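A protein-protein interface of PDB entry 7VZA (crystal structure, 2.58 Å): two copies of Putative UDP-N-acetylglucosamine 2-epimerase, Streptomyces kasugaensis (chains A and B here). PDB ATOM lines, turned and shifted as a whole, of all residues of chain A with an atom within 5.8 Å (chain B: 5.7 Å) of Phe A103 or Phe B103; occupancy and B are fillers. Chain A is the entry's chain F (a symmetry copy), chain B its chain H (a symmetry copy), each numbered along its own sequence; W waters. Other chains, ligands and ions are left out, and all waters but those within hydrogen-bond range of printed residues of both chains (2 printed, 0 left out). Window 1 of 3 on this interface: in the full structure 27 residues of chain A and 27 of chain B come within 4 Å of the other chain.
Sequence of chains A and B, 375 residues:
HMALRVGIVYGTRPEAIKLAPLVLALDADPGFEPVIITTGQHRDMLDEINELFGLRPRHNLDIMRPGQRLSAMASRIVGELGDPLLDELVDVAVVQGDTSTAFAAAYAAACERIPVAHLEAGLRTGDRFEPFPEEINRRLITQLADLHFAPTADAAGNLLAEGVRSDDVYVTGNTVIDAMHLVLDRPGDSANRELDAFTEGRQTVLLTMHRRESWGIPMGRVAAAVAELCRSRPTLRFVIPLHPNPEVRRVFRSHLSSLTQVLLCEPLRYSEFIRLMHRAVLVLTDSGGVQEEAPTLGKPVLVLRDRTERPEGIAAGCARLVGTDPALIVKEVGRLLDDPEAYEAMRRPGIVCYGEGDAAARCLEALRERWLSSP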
ATOM      1  N   ALA A  74      -5.810  24.729  -5.856  1.00  0.00           N
ATOM      2  CA  ALA A  74      -4.526  24.027  -5.595  1.00  0.00           C
ATOM      3  C   ALA A  74      -4.650  22.569  -6.041  1.00  0.00           C
ATOM      4  O   ALA A  74      -3.767  22.079  -6.757  1.00  0.00           O
ATOM      5  CB  ALA A  74      -4.165  24.121  -4.128  1.00  0.00           C
ATOM      6  N   VAL A  95       8.754  29.164 -11.412  1.00  0.00           N
ATOM      7  CA  VAL A  95       7.540  29.836 -10.865  1.00  0.00           C
ATOM      8  C   VAL A  95       7.998  31.169 -10.285  1.00  0.00           C
ATOM      9  O   VAL A  95       9.179  31.277  -9.918  1.00  0.00           O
ATOM     10  CB  VAL A  95       6.838  28.969  -9.812  1.00  0.00           C
ATOM     11  CG1 VAL A  95       6.409  27.635 -10.396  1.00  0.00           C
ATOM     12  CG2 VAL A  95       7.701  28.761  -8.565  1.00  0.00           C
ATOM     13  N   THR A  99       2.287  33.488  -5.339  1.00  0.00           N
ATOM     14  CA  THR A  99       0.924  33.079  -5.774  1.00  0.00           C
ATOM     15  C   THR A  99       0.691  31.610  -5.411  1.00  0.00           C
ATOM     16  O   THR A  99       1.667  30.845  -5.333  1.00  0.00           O
ATOM     17  CB  THR A  99       0.711  33.323  -7.271  1.00  0.00           C
ATOM     18  OG1 THR A  99       1.539  32.416  -7.998  1.00  0.00           O
ATOM     19  CG2 THR A  99       1.033  34.743  -7.681  1.00  0.00           C
ATOM     20  N   SER A 100      -0.565  31.224  -5.220  1.00  0.00           N
ATOM     21  CA  SER A 100      -0.955  29.819  -4.953  1.00  0.00           C
ATOM     22  C   SER A 100      -0.646  28.959  -6.188  1.00  0.00           C
ATOM     23  O   SER A 100      -0.392  27.748  -6.016  1.00  0.00           O
ATOM     24  CB  SER A 100      -2.384  29.729  -4.506  1.00  0.00           C
ATOM     25  OG  SER A 100      -2.537  30.301  -3.209  1.00  0.00           O
ATOM     26  N   THR A 101      -0.610  29.568  -7.376  1.00  0.00           N
ATOM     27  CA  THR A 101      -0.175  28.900  -8.626  1.00  0.00           C
ATOM     28  C   THR A 101       1.294  28.498  -8.494  1.00  0.00           C
ATOM     29  O   THR A 101       1.611  27.321  -8.727  1.00  0.00           O
ATOM     30  CB  THR A 101      -0.418  29.781  -9.863  1.00  0.00           C
ATOM     31  OG1 THR A 101      -1.808  29.717 -10.182  1.00  0.00           O
ATOM     32  CG2 THR A 101       0.362  29.335 -11.080  1.00  0.00           C
ATOM     33  N   ALA A 102       2.162  29.446  -8.140  1.00  0.00           N
ATOM     34  CA  ALA A 102       3.617  29.211  -8.019  1.00  0.00           C
ATOM     35  C   ALA A 102       3.853  28.035  -7.073  1.00  0.00           C
ATOM     36  O   ALA A 102       4.685  27.175  -7.388  1.00  0.00           O
ATOM     37  CB  ALA A 102       4.317  30.444  -7.539  1.00  0.00           C
ATOM     38  N   PHE A 103       3.124  27.975  -5.964  1.00  0.00           N
ATOM     39  CA  PHE A 103       3.276  26.871  -4.985  1.00  0.00           C
ATOM     40  C   PHE A 103       2.774  25.556  -5.582  1.00  0.00           C
ATOM     41  O   PHE A 103       3.539  24.579  -5.615  1.00  0.00           O
ATOM     42  CB  PHE A 103       2.517  27.140  -3.692  1.00  0.00           C
ATOM     43  CG  PHE A 103       2.327  25.875  -2.912  1.00  0.00           C
ATOM     44  CD1 PHE A 103       3.432  25.172  -2.472  1.00  0.00           C
ATOM     45  CD2 PHE A 103       1.067  25.355  -2.693  1.00  0.00           C
ATOM     46  CE1 PHE A 103       3.278  23.985  -1.780  1.00  0.00           C
ATOM     47  CE2 PHE A 103       0.913  24.180  -1.983  1.00  0.00           C
ATOM     48  CZ  PHE A 103       2.017  23.499  -1.528  1.00  0.00           C
ATOM     49  N   ALA A 104       1.515  25.510  -6.014  1.00  0.00           N
ATOM     50  CA  ALA A 104       0.884  24.270  -6.519  1.00  0.00           C
ATOM     51  C   ALA A 104       1.660  23.750  -7.731  1.00  0.00           C
ATOM     52  O   ALA A 104       1.898  22.535  -7.798  1.00  0.00           O
ATOM     53  CB  ALA A 104      -0.570  24.497  -6.840  1.00  0.00           C
ATOM     54  N   ALA A 105       2.059  24.628  -8.650  1.00  0.00           N
ATOM     55  CA  ALA A 105       2.856  24.265  -9.847  1.00  0.00           C
ATOM     56  C   ALA A 105       4.199  23.680  -9.414  1.00  0.00           C
ATOM     57  O   ALA A 105       4.619  22.661  -9.982  1.00  0.00           O
ATOM     58  CB  ALA A 105       3.046  25.448 -10.741  1.00  0.00           C
ATOM     59  N   ALA A 106       4.862  24.305  -8.443  1.00  0.00           N
ATOM     60  CA  ALA A 106       6.170  23.837  -7.940  1.00  0.00           C
ATOM     61  C   ALA A 106       5.986  22.432  -7.358  1.00  0.00           C
ATOM     62  O   ALA A 106       6.801  21.554  -7.672  1.00  0.00           O
ATOM     63  CB  ALA A 106       6.741  24.819  -6.949  1.00  0.00           C
ATOM     64  N   TYR A 107       4.934  22.200  -6.573  1.00  0.00           N
ATOM     65  CA  TYR A 107       4.653  20.865  -5.985  1.00  0.00           C
ATOM     66  C   TYR A 107       4.421  19.850  -7.112  1.00  0.00           C
ATOM     67  O   TYR A 107       4.993  18.741  -7.048  1.00  0.00           O
ATOM     68  CB  TYR A 107       3.477  20.877  -5.007  1.00  0.00           C
ATOM     69  CG  TYR A 107       3.301  19.536  -4.349  1.00  0.00           C
ATOM     70  CD1 TYR A 107       4.214  19.076  -3.417  1.00  0.00           C
ATOM     71  CD2 TYR A 107       2.301  18.672  -4.744  1.00  0.00           C
ATOM     72  CE1 TYR A 107       4.107  17.815  -2.854  1.00  0.00           C
ATOM     73  CE2 TYR A 107       2.168  17.411  -4.184  1.00  0.00           C
ATOM     74  CZ  TYR A 107       3.068  16.984  -3.226  1.00  0.00           C
ATOM     75  OH  TYR A 107       2.946  15.742  -2.673  1.00  0.00           O
ATOM     76  N   ALA A 108       3.617  20.209  -8.118  1.00  0.00           N
ATOM     77  CA  ALA A 108       3.329  19.348  -9.290  1.00  0.00           C
ATOM     78  C   ALA A 108       4.640  18.985  -9.981  1.00  0.00           C
ATOM     79  O   ALA A 108       4.849  17.801 -10.279  1.00  0.00           O
ATOM     80  CB  ALA A 108       2.395  20.039 -10.251  1.00  0.00           C
ATOM     81  N   ASN A 137       3.056  30.510   1.092  1.00  0.00           N
ATOM     82  CA  ASN A 137       3.405  30.058  -0.278  1.00  0.00           C
ATOM     83  C   ASN A 137       4.914  30.217  -0.508  1.00  0.00           C
ATOM     84  O   ASN A 137       5.546  29.243  -0.962  1.00  0.00           O
ATOM     85  CB  ASN A 137       2.639  30.838  -1.345  1.00  0.00           C
ATOM     86  CG  ASN A 137       1.182  30.440  -1.450  1.00  0.00           C
ATOM     87  OD1 ASN A 137       0.791  29.350  -1.043  1.00  0.00           O
ATOM     88  ND2 ASN A 137       0.374  31.321  -2.011  1.00  0.00           N
ATOM     89  N   LEU A 140       6.888  27.633   1.379  1.00  0.00           N
ATOM     90  CA  LEU A 140       6.696  26.278   0.800  1.00  0.00           C
ATOM     91  C   LEU A 140       7.495  26.174  -0.508  1.00  0.00           C
ATOM     92  O   LEU A 140       8.216  25.178  -0.681  1.00  0.00           O
ATOM     93  CB  LEU A 140       5.206  26.025   0.561  1.00  0.00           C
ATOM     94  CG  LEU A 140       4.356  25.789   1.806  1.00  0.00           C
ATOM     95  CD1 LEU A 140       2.886  25.699   1.428  1.00  0.00           C
ATOM     96  CD2 LEU A 140       4.787  24.532   2.551  1.00  0.00           C
ATOM     97  N   ILE A 141       7.365  27.160  -1.399  1.00  0.00           N
ATOM     98  CA  ILE A 141       8.121  27.196  -2.683  1.00  0.00           C
ATOM     99  C   ILE A 141       9.608  27.123  -2.352  1.00  0.00           C
ATOM    100  O   ILE A 141      10.341  26.435  -3.078  1.00  0.00           O
ATOM    101  CB  ILE A 141       7.807  28.455  -3.517  1.00  0.00           C
ATOM    102  CG1 ILE A 141       6.355  28.502  -3.987  1.00  0.00           C
ATOM    103  CG2 ILE A 141       8.761  28.577  -4.690  1.00  0.00           C
ATOM    104  CD1 ILE A 141       5.869  29.892  -4.315  1.00  0.00           C
ATOM    105  N   LEU A 144      10.773  23.689  -1.947  1.00  0.00           N
ATOM    106  CA  LEU A 144      10.586  22.877  -3.184  1.00  0.00           C
ATOM    107  C   LEU A 144      11.669  23.241  -4.209  1.00  0.00           C
ATOM    108  O   LEU A 144      12.173  22.319  -4.879  1.00  0.00           O
ATOM    109  CB  LEU A 144       9.187  23.109  -3.761  1.00  0.00           C
ATOM    110  CG  LEU A 144       8.054  22.410  -3.018  1.00  0.00           C
ATOM    111  CD1 LEU A 144       6.713  23.069  -3.297  1.00  0.00           C
ATOM    112  CD2 LEU A 144       8.006  20.924  -3.340  1.00  0.00           C
ATOM    113  N   ALA B  74      -2.111  13.405  -3.765  1.00  0.00           N
ATOM    114  CA  ALA B  74      -1.972  14.725  -3.103  1.00  0.00           C
ATOM    115  C   ALA B  74      -3.145  15.615  -3.527  1.00  0.00           C
ATOM    116  O   ALA B  74      -3.784  16.225  -2.649  1.00  0.00           O
ATOM    117  CB  ALA B  74      -0.649  15.358  -3.457  1.00  0.00           C
ATOM    118  N   VAL B  95      -0.792  16.109  12.268  1.00  0.00           N
ATOM    119  CA  VAL B  95      -0.274  15.123  11.276  1.00  0.00           C
ATOM    120  C   VAL B  95       1.026  14.562  11.847  1.00  0.00           C
ATOM    121  O   VAL B  95       1.660  15.257  12.665  1.00  0.00           O
ATOM    122  CB  VAL B  95      -0.062  15.768   9.897  1.00  0.00           C
ATOM    123  CG1 VAL B  95      -1.364  16.343   9.345  1.00  0.00           C
ATOM    124  CG2 VAL B  95       1.030  16.825   9.913  1.00  0.00           C
ATOM    125  N   THR B  99       4.931  11.395   5.763  1.00  0.00           N
ATOM    126  CA  THR B  99       4.039  10.797   4.732  1.00  0.00           C
ATOM    127  C   THR B  99       3.478  11.905   3.833  1.00  0.00           C
ATOM    128  O   THR B  99       3.352  13.054   4.305  1.00  0.00           O
ATOM    129  CB  THR B  99       2.910   9.976   5.371  1.00  0.00           C
ATOM    130  OG1 THR B  99       2.015  10.866   6.043  1.00  0.00           O
ATOM    131  CG2 THR B  99       3.429   8.943   6.347  1.00  0.00           C
ATOM    132  N   SER B 100       3.132  11.568   2.596  1.00  0.00           N
ATOM    133  CA  SER B 100       2.491  12.515   1.648  1.00  0.00           C
ATOM    134  C   SER B 100       1.097  12.900   2.165  1.00  0.00           C
ATOM    135  O   SER B 100       0.630  14.011   1.844  1.00  0.00           O
ATOM    136  CB  SER B 100       2.464  11.963   0.251  1.00  0.00           C
ATOM    137  OG  SER B 100       3.776  11.916  -0.287  1.00  0.00           O
ATOM    138  N   THR B 101       0.482  12.048   2.985  1.00  0.00           N
ATOM    139  CA  THR B 101      -0.797  12.357   3.682  1.00  0.00           C
ATOM    140  C   THR B 101      -0.563  13.523   4.648  1.00  0.00           C
ATOM    141  O   THR B 101      -1.316  14.506   4.573  1.00  0.00           O
ATOM    142  CB  THR B 101      -1.365  11.132   4.407  1.00  0.00           C
ATOM    143  OG1 THR B 101      -1.975  10.318   3.414  1.00  0.00           O
ATOM    144  CG2 THR B 101      -2.399  11.478   5.452  1.00  0.00           C
ATOM    145  N   ALA B 102       0.442  13.414   5.520  1.00  0.00           N
ATOM    146  CA  ALA B 102       0.742  14.436   6.540  1.00  0.00           C
ATOM    147  C   ALA B 102       0.922  15.784   5.850  1.00  0.00           C
ATOM    148  O   ALA B 102       0.393  16.781   6.355  1.00  0.00           O
ATOM    149  CB  ALA B 102       1.962  14.047   7.328  1.00  0.00           C
ATOM    150  N   PHE B 103       1.620  15.811   4.714  1.00  0.00           N
ATOM    151  CA  PHE B 103       1.844  17.067   3.966  1.00  0.00           C
ATOM    152  C   PHE B 103       0.532  17.576   3.366  1.00  0.00           C
ATOM    153  O   PHE B 103       0.142  18.731   3.638  1.00  0.00           O
ATOM    154  CB  PHE B 103       2.854  16.896   2.838  1.00  0.00           C
ATOM    155  CG  PHE B 103       2.756  18.032   1.862  1.00  0.00           C
ATOM    156  CD1 PHE B 103       2.969  19.329   2.287  1.00  0.00           C
ATOM    157  CD2 PHE B 103       2.364  17.805   0.557  1.00  0.00           C
ATOM    158  CE1 PHE B 103       2.851  20.381   1.398  1.00  0.00           C
ATOM    159  CE2 PHE B 103       2.238  18.861  -0.326  1.00  0.00           C
ATOM    160  CZ  PHE B 103       2.484  20.146   0.100  1.00  0.00           C
ATOM    161  N   ALA B 104      -0.131  16.763   2.543  1.00  0.00           N
ATOM    162  CA  ALA B 104      -1.353  17.181   1.815  1.00  0.00           C
ATOM    163  C   ALA B 104      -2.445  17.566   2.816  1.00  0.00           C
ATOM    164  O   ALA B 104      -3.106  18.596   2.592  1.00  0.00           O
ATOM    165  CB  ALA B 104      -1.812  16.108   0.872  1.00  0.00           C
ATOM    166  N   ALA B 105      -2.615  16.798   3.894  1.00  0.00           N
ATOM    167  CA  ALA B 105      -3.601  17.091   4.964  1.00  0.00           C
ATOM    168  C   ALA B 105      -3.266  18.426   5.625  1.00  0.00           C
ATOM    169  O   ALA B 105      -4.186  19.224   5.856  1.00  0.00           O
ATOM    170  CB  ALA B 105      -3.629  15.996   5.990  1.00  0.00           C
ATOM    171  N   ALA B 106      -1.993  18.663   5.930  1.00  0.00           N
ATOM    172  CA  ALA B 106      -1.546  19.920   6.570  1.00  0.00           C
ATOM    173  C   ALA B 106      -1.880  21.086   5.630  1.00  0.00           C
ATOM    174  O   ALA B 106      -2.424  22.086   6.109  1.00  0.00           O
ATOM    175  CB  ALA B 106      -0.078  19.857   6.917  1.00  0.00           C
ATOM    176  N   TYR B 107      -1.614  20.956   4.332  1.00  0.00           N
ATOM    177  CA  TYR B 107      -1.939  22.017   3.346  1.00  0.00           C
ATOM    178  C   TYR B 107      -3.458  22.258   3.322  1.00  0.00           C
ATOM    179  O   TYR B 107      -3.886  23.428   3.350  1.00  0.00           O
ATOM    180  CB  TYR B 107      -1.407  21.719   1.942  1.00  0.00           C
ATOM    181  CG  TYR B 107      -1.648  22.889   1.021  1.00  0.00           C
ATOM    182  CD1 TYR B 107      -0.937  24.068   1.170  1.00  0.00           C
ATOM    183  CD2 TYR B 107      -2.665  22.866   0.083  1.00  0.00           C
ATOM    184  CE1 TYR B 107      -1.197  25.177   0.383  1.00  0.00           C
ATOM    185  CE2 TYR B 107      -2.932  23.959  -0.725  1.00  0.00           C
ATOM    186  CZ  TYR B 107      -2.198  25.126  -0.572  1.00  0.00           C
ATOM    187  OH  TYR B 107      -2.433  26.224  -1.347  1.00  0.00           O
ATOM    188  N   ALA B 108      -4.252  21.188   3.282  1.00  0.00           N
ATOM    189  CA  ALA B 108      -5.734  21.263   3.304  1.00  0.00           C
ATOM    190  C   ALA B 108      -6.189  22.010   4.560  1.00  0.00           C
ATOM    191  O   ALA B 108      -7.024  22.915   4.448  1.00  0.00           O
ATOM    192  CB  ALA B 108      -6.339  19.890   3.243  1.00  0.00           C
ATOM    193  N   ASN B 137       8.698  16.297   2.209  1.00  0.00           N
ATOM    194  CA  ASN B 137       7.438  16.352   2.992  1.00  0.00           C
ATOM    195  C   ASN B 137       7.692  16.976   4.365  1.00  0.00           C
ATOM    196  O   ASN B 137       6.948  17.896   4.736  1.00  0.00           O
ATOM    197  CB  ASN B 137       6.807  14.973   3.168  1.00  0.00           C
ATOM    198  CG  ASN B 137       6.157  14.446   1.911  1.00  0.00           C
ATOM    199  OD1 ASN B 137       5.808  15.210   1.009  1.00  0.00           O
ATOM    200  ND2 ASN B 137       5.987  13.137   1.855  1.00  0.00           N
ATOM    201  N   LEU B 140       8.258  20.678   4.079  1.00  0.00           N
ATOM    202  CA  LEU B 140       6.999  21.383   3.712  1.00  0.00           C
ATOM    203  C   LEU B 140       6.081  21.444   4.940  1.00  0.00           C
ATOM    204  O   LEU B 140       5.555  22.540   5.224  1.00  0.00           O
ATOM    205  CB  LEU B 140       6.314  20.655   2.551  1.00  0.00           C
ATOM    206  CG  LEU B 140       6.978  20.798   1.187  1.00  0.00           C
ATOM    207  CD1 LEU B 140       6.274  19.910   0.173  1.00  0.00           C
ATOM    208  CD2 LEU B 140       6.977  22.242   0.711  1.00  0.00           C
ATOM    209  N   ILE B 141       5.882  20.318   5.629  1.00  0.00           N
ATOM    210  CA  ILE B 141       5.044  20.265   6.859  1.00  0.00           C
ATOM    211  C   ILE B 141       5.619  21.268   7.856  1.00  0.00           C
ATOM    212  O   ILE B 141       4.833  21.945   8.536  1.00  0.00           O
ATOM    213  CB  ILE B 141       4.984  18.851   7.466  1.00  0.00           C
ATOM    214  CG1 ILE B 141       4.282  17.850   6.541  1.00  0.00           C
ATOM    215  CG2 ILE B 141       4.320  18.884   8.836  1.00  0.00           C
ATOM    216  CD1 ILE B 141       4.645  16.411   6.822  1.00  0.00           C
ATOM    217  N   LEU B 144       4.355  24.659   7.319  1.00  0.00           N
ATOM    218  CA  LEU B 144       2.876  24.747   7.488  1.00  0.00           C
ATOM    219  C   LEU B 144       2.511  24.724   8.978  1.00  0.00           C
ATOM    220  O   LEU B 144       1.594  25.479   9.367  1.00  0.00           O
ATOM    221  CB  LEU B 144       2.200  23.598   6.733  1.00  0.00           C
ATOM    222  CG  LEU B 144       2.127  23.785   5.222  1.00  0.00           C
ATOM    223  CD1 LEU B 144       1.915  22.447   4.528  1.00  0.00           C
ATOM    224  CD2 LEU B 144       1.012  24.759   4.856  1.00  0.00           C
HETATM  225  O   HOH W   1      -1.539  28.644  -1.397  1.00  0.00           O
HETATM  226  O   HOH W   2       4.425  14.185  -1.045  1.00  0.00           O
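Hydrophobic or aromatic side chains of chain A within 4 Å of the printed part of chain B: Ala A74, Phe A103, Tyr A107, Leu A140 and Leu A144. Of the 16 printed residues of chain B, 5 touch a printed residue of chain A. Printed residues of chain B that touch a printed residue of chain A: Ala B74, Phe B103, Tyr B107, Leu B140 and Leu B144. Hydrophobic or aromatic side chains of chain B that line the printed part of chain A: Ala B74, Phe B103, Tyr B107, Leu B140 and Leu B144. Among the printed residues, 8 pairs touch across the chains.
Ala A74 touches Tyr B107 (CB to CE2, 3.6 Å). Phe B103 touches Phe A103 (CZ to CZ, 3.8 Å). CE2 of Phe A103 touches CE1 of Tyr B107 (3.3 Å). CE2 of Tyr A107 touches CB of Ala B74 (3.6 Å). Phe B103 touches Tyr A107 (CE2 to CE1, 3.3 Å). CD2 of Leu A140 touches O of Leu B140 (3.4 Å). CD2 of Leu A140 touches CG of Leu B144 (3.8 Å). Leu A144 touches Leu B140.
Water W1 lies within hydrogen-bond range of the side-chain amide oxygen (OD1) of Asn A137 (2.5 Å), the side-chain hydroxyl (OH) of Tyr B107 (2.6 Å) and the side-chain hydroxyl (OG) of Ser A100 (2.7 Å). Water W2 lies within hydrogen-bond range of the side-chain hydroxyl of Ser B100 (2.5 Å), the side-chain amide oxygen of Asn B137 (2.7 Å) and the side-chain hydroxyl of Tyr A107 (2.7 Å).
Phe A103 touches just these residues of chain B: Phe B103 (3.8 Å) and Tyr B107 (3.3 Å). Of chain A, only Phe A103 and Tyr A107 come within 4 Å of Phe B103. Of the printed residues of chain A, Leu B140 touches Leu A140 and Leu A144. Of the printed residues of chain A, Tyr B107 touches Ala A74 (3.6 Å) and Phe A103 (3.3 Å). Printed residues of chain B within 4 Å of Tyr A107: Ala B74 (3.6 Å) and Phe B103 (3.3 Å). Thr A101 touches none of the printed residues of chain B. The nearest residue of chain B that does not touch Phe A103 is Leu B140 (4.8 Å). The nearest residue of chain A that does not touch Phe B103 is Leu A140 (4.7 Å).
Ala A74 touches Tyr B107, and with the chains exchanged Tyr A107 touches Ala B74. Phe A103 touches its own counterpart, Phe B103. Leu A140 touches its own counterpart, Leu B140. Leu A140 touches Leu B144, and with the chains exchanged Leu A144 touches Leu B140. Positions printed for both chains: 74, 95, 99, 100, 101, 102, 103, 104, 105, 106, 107, 108, 137, 140, 141 and 144.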
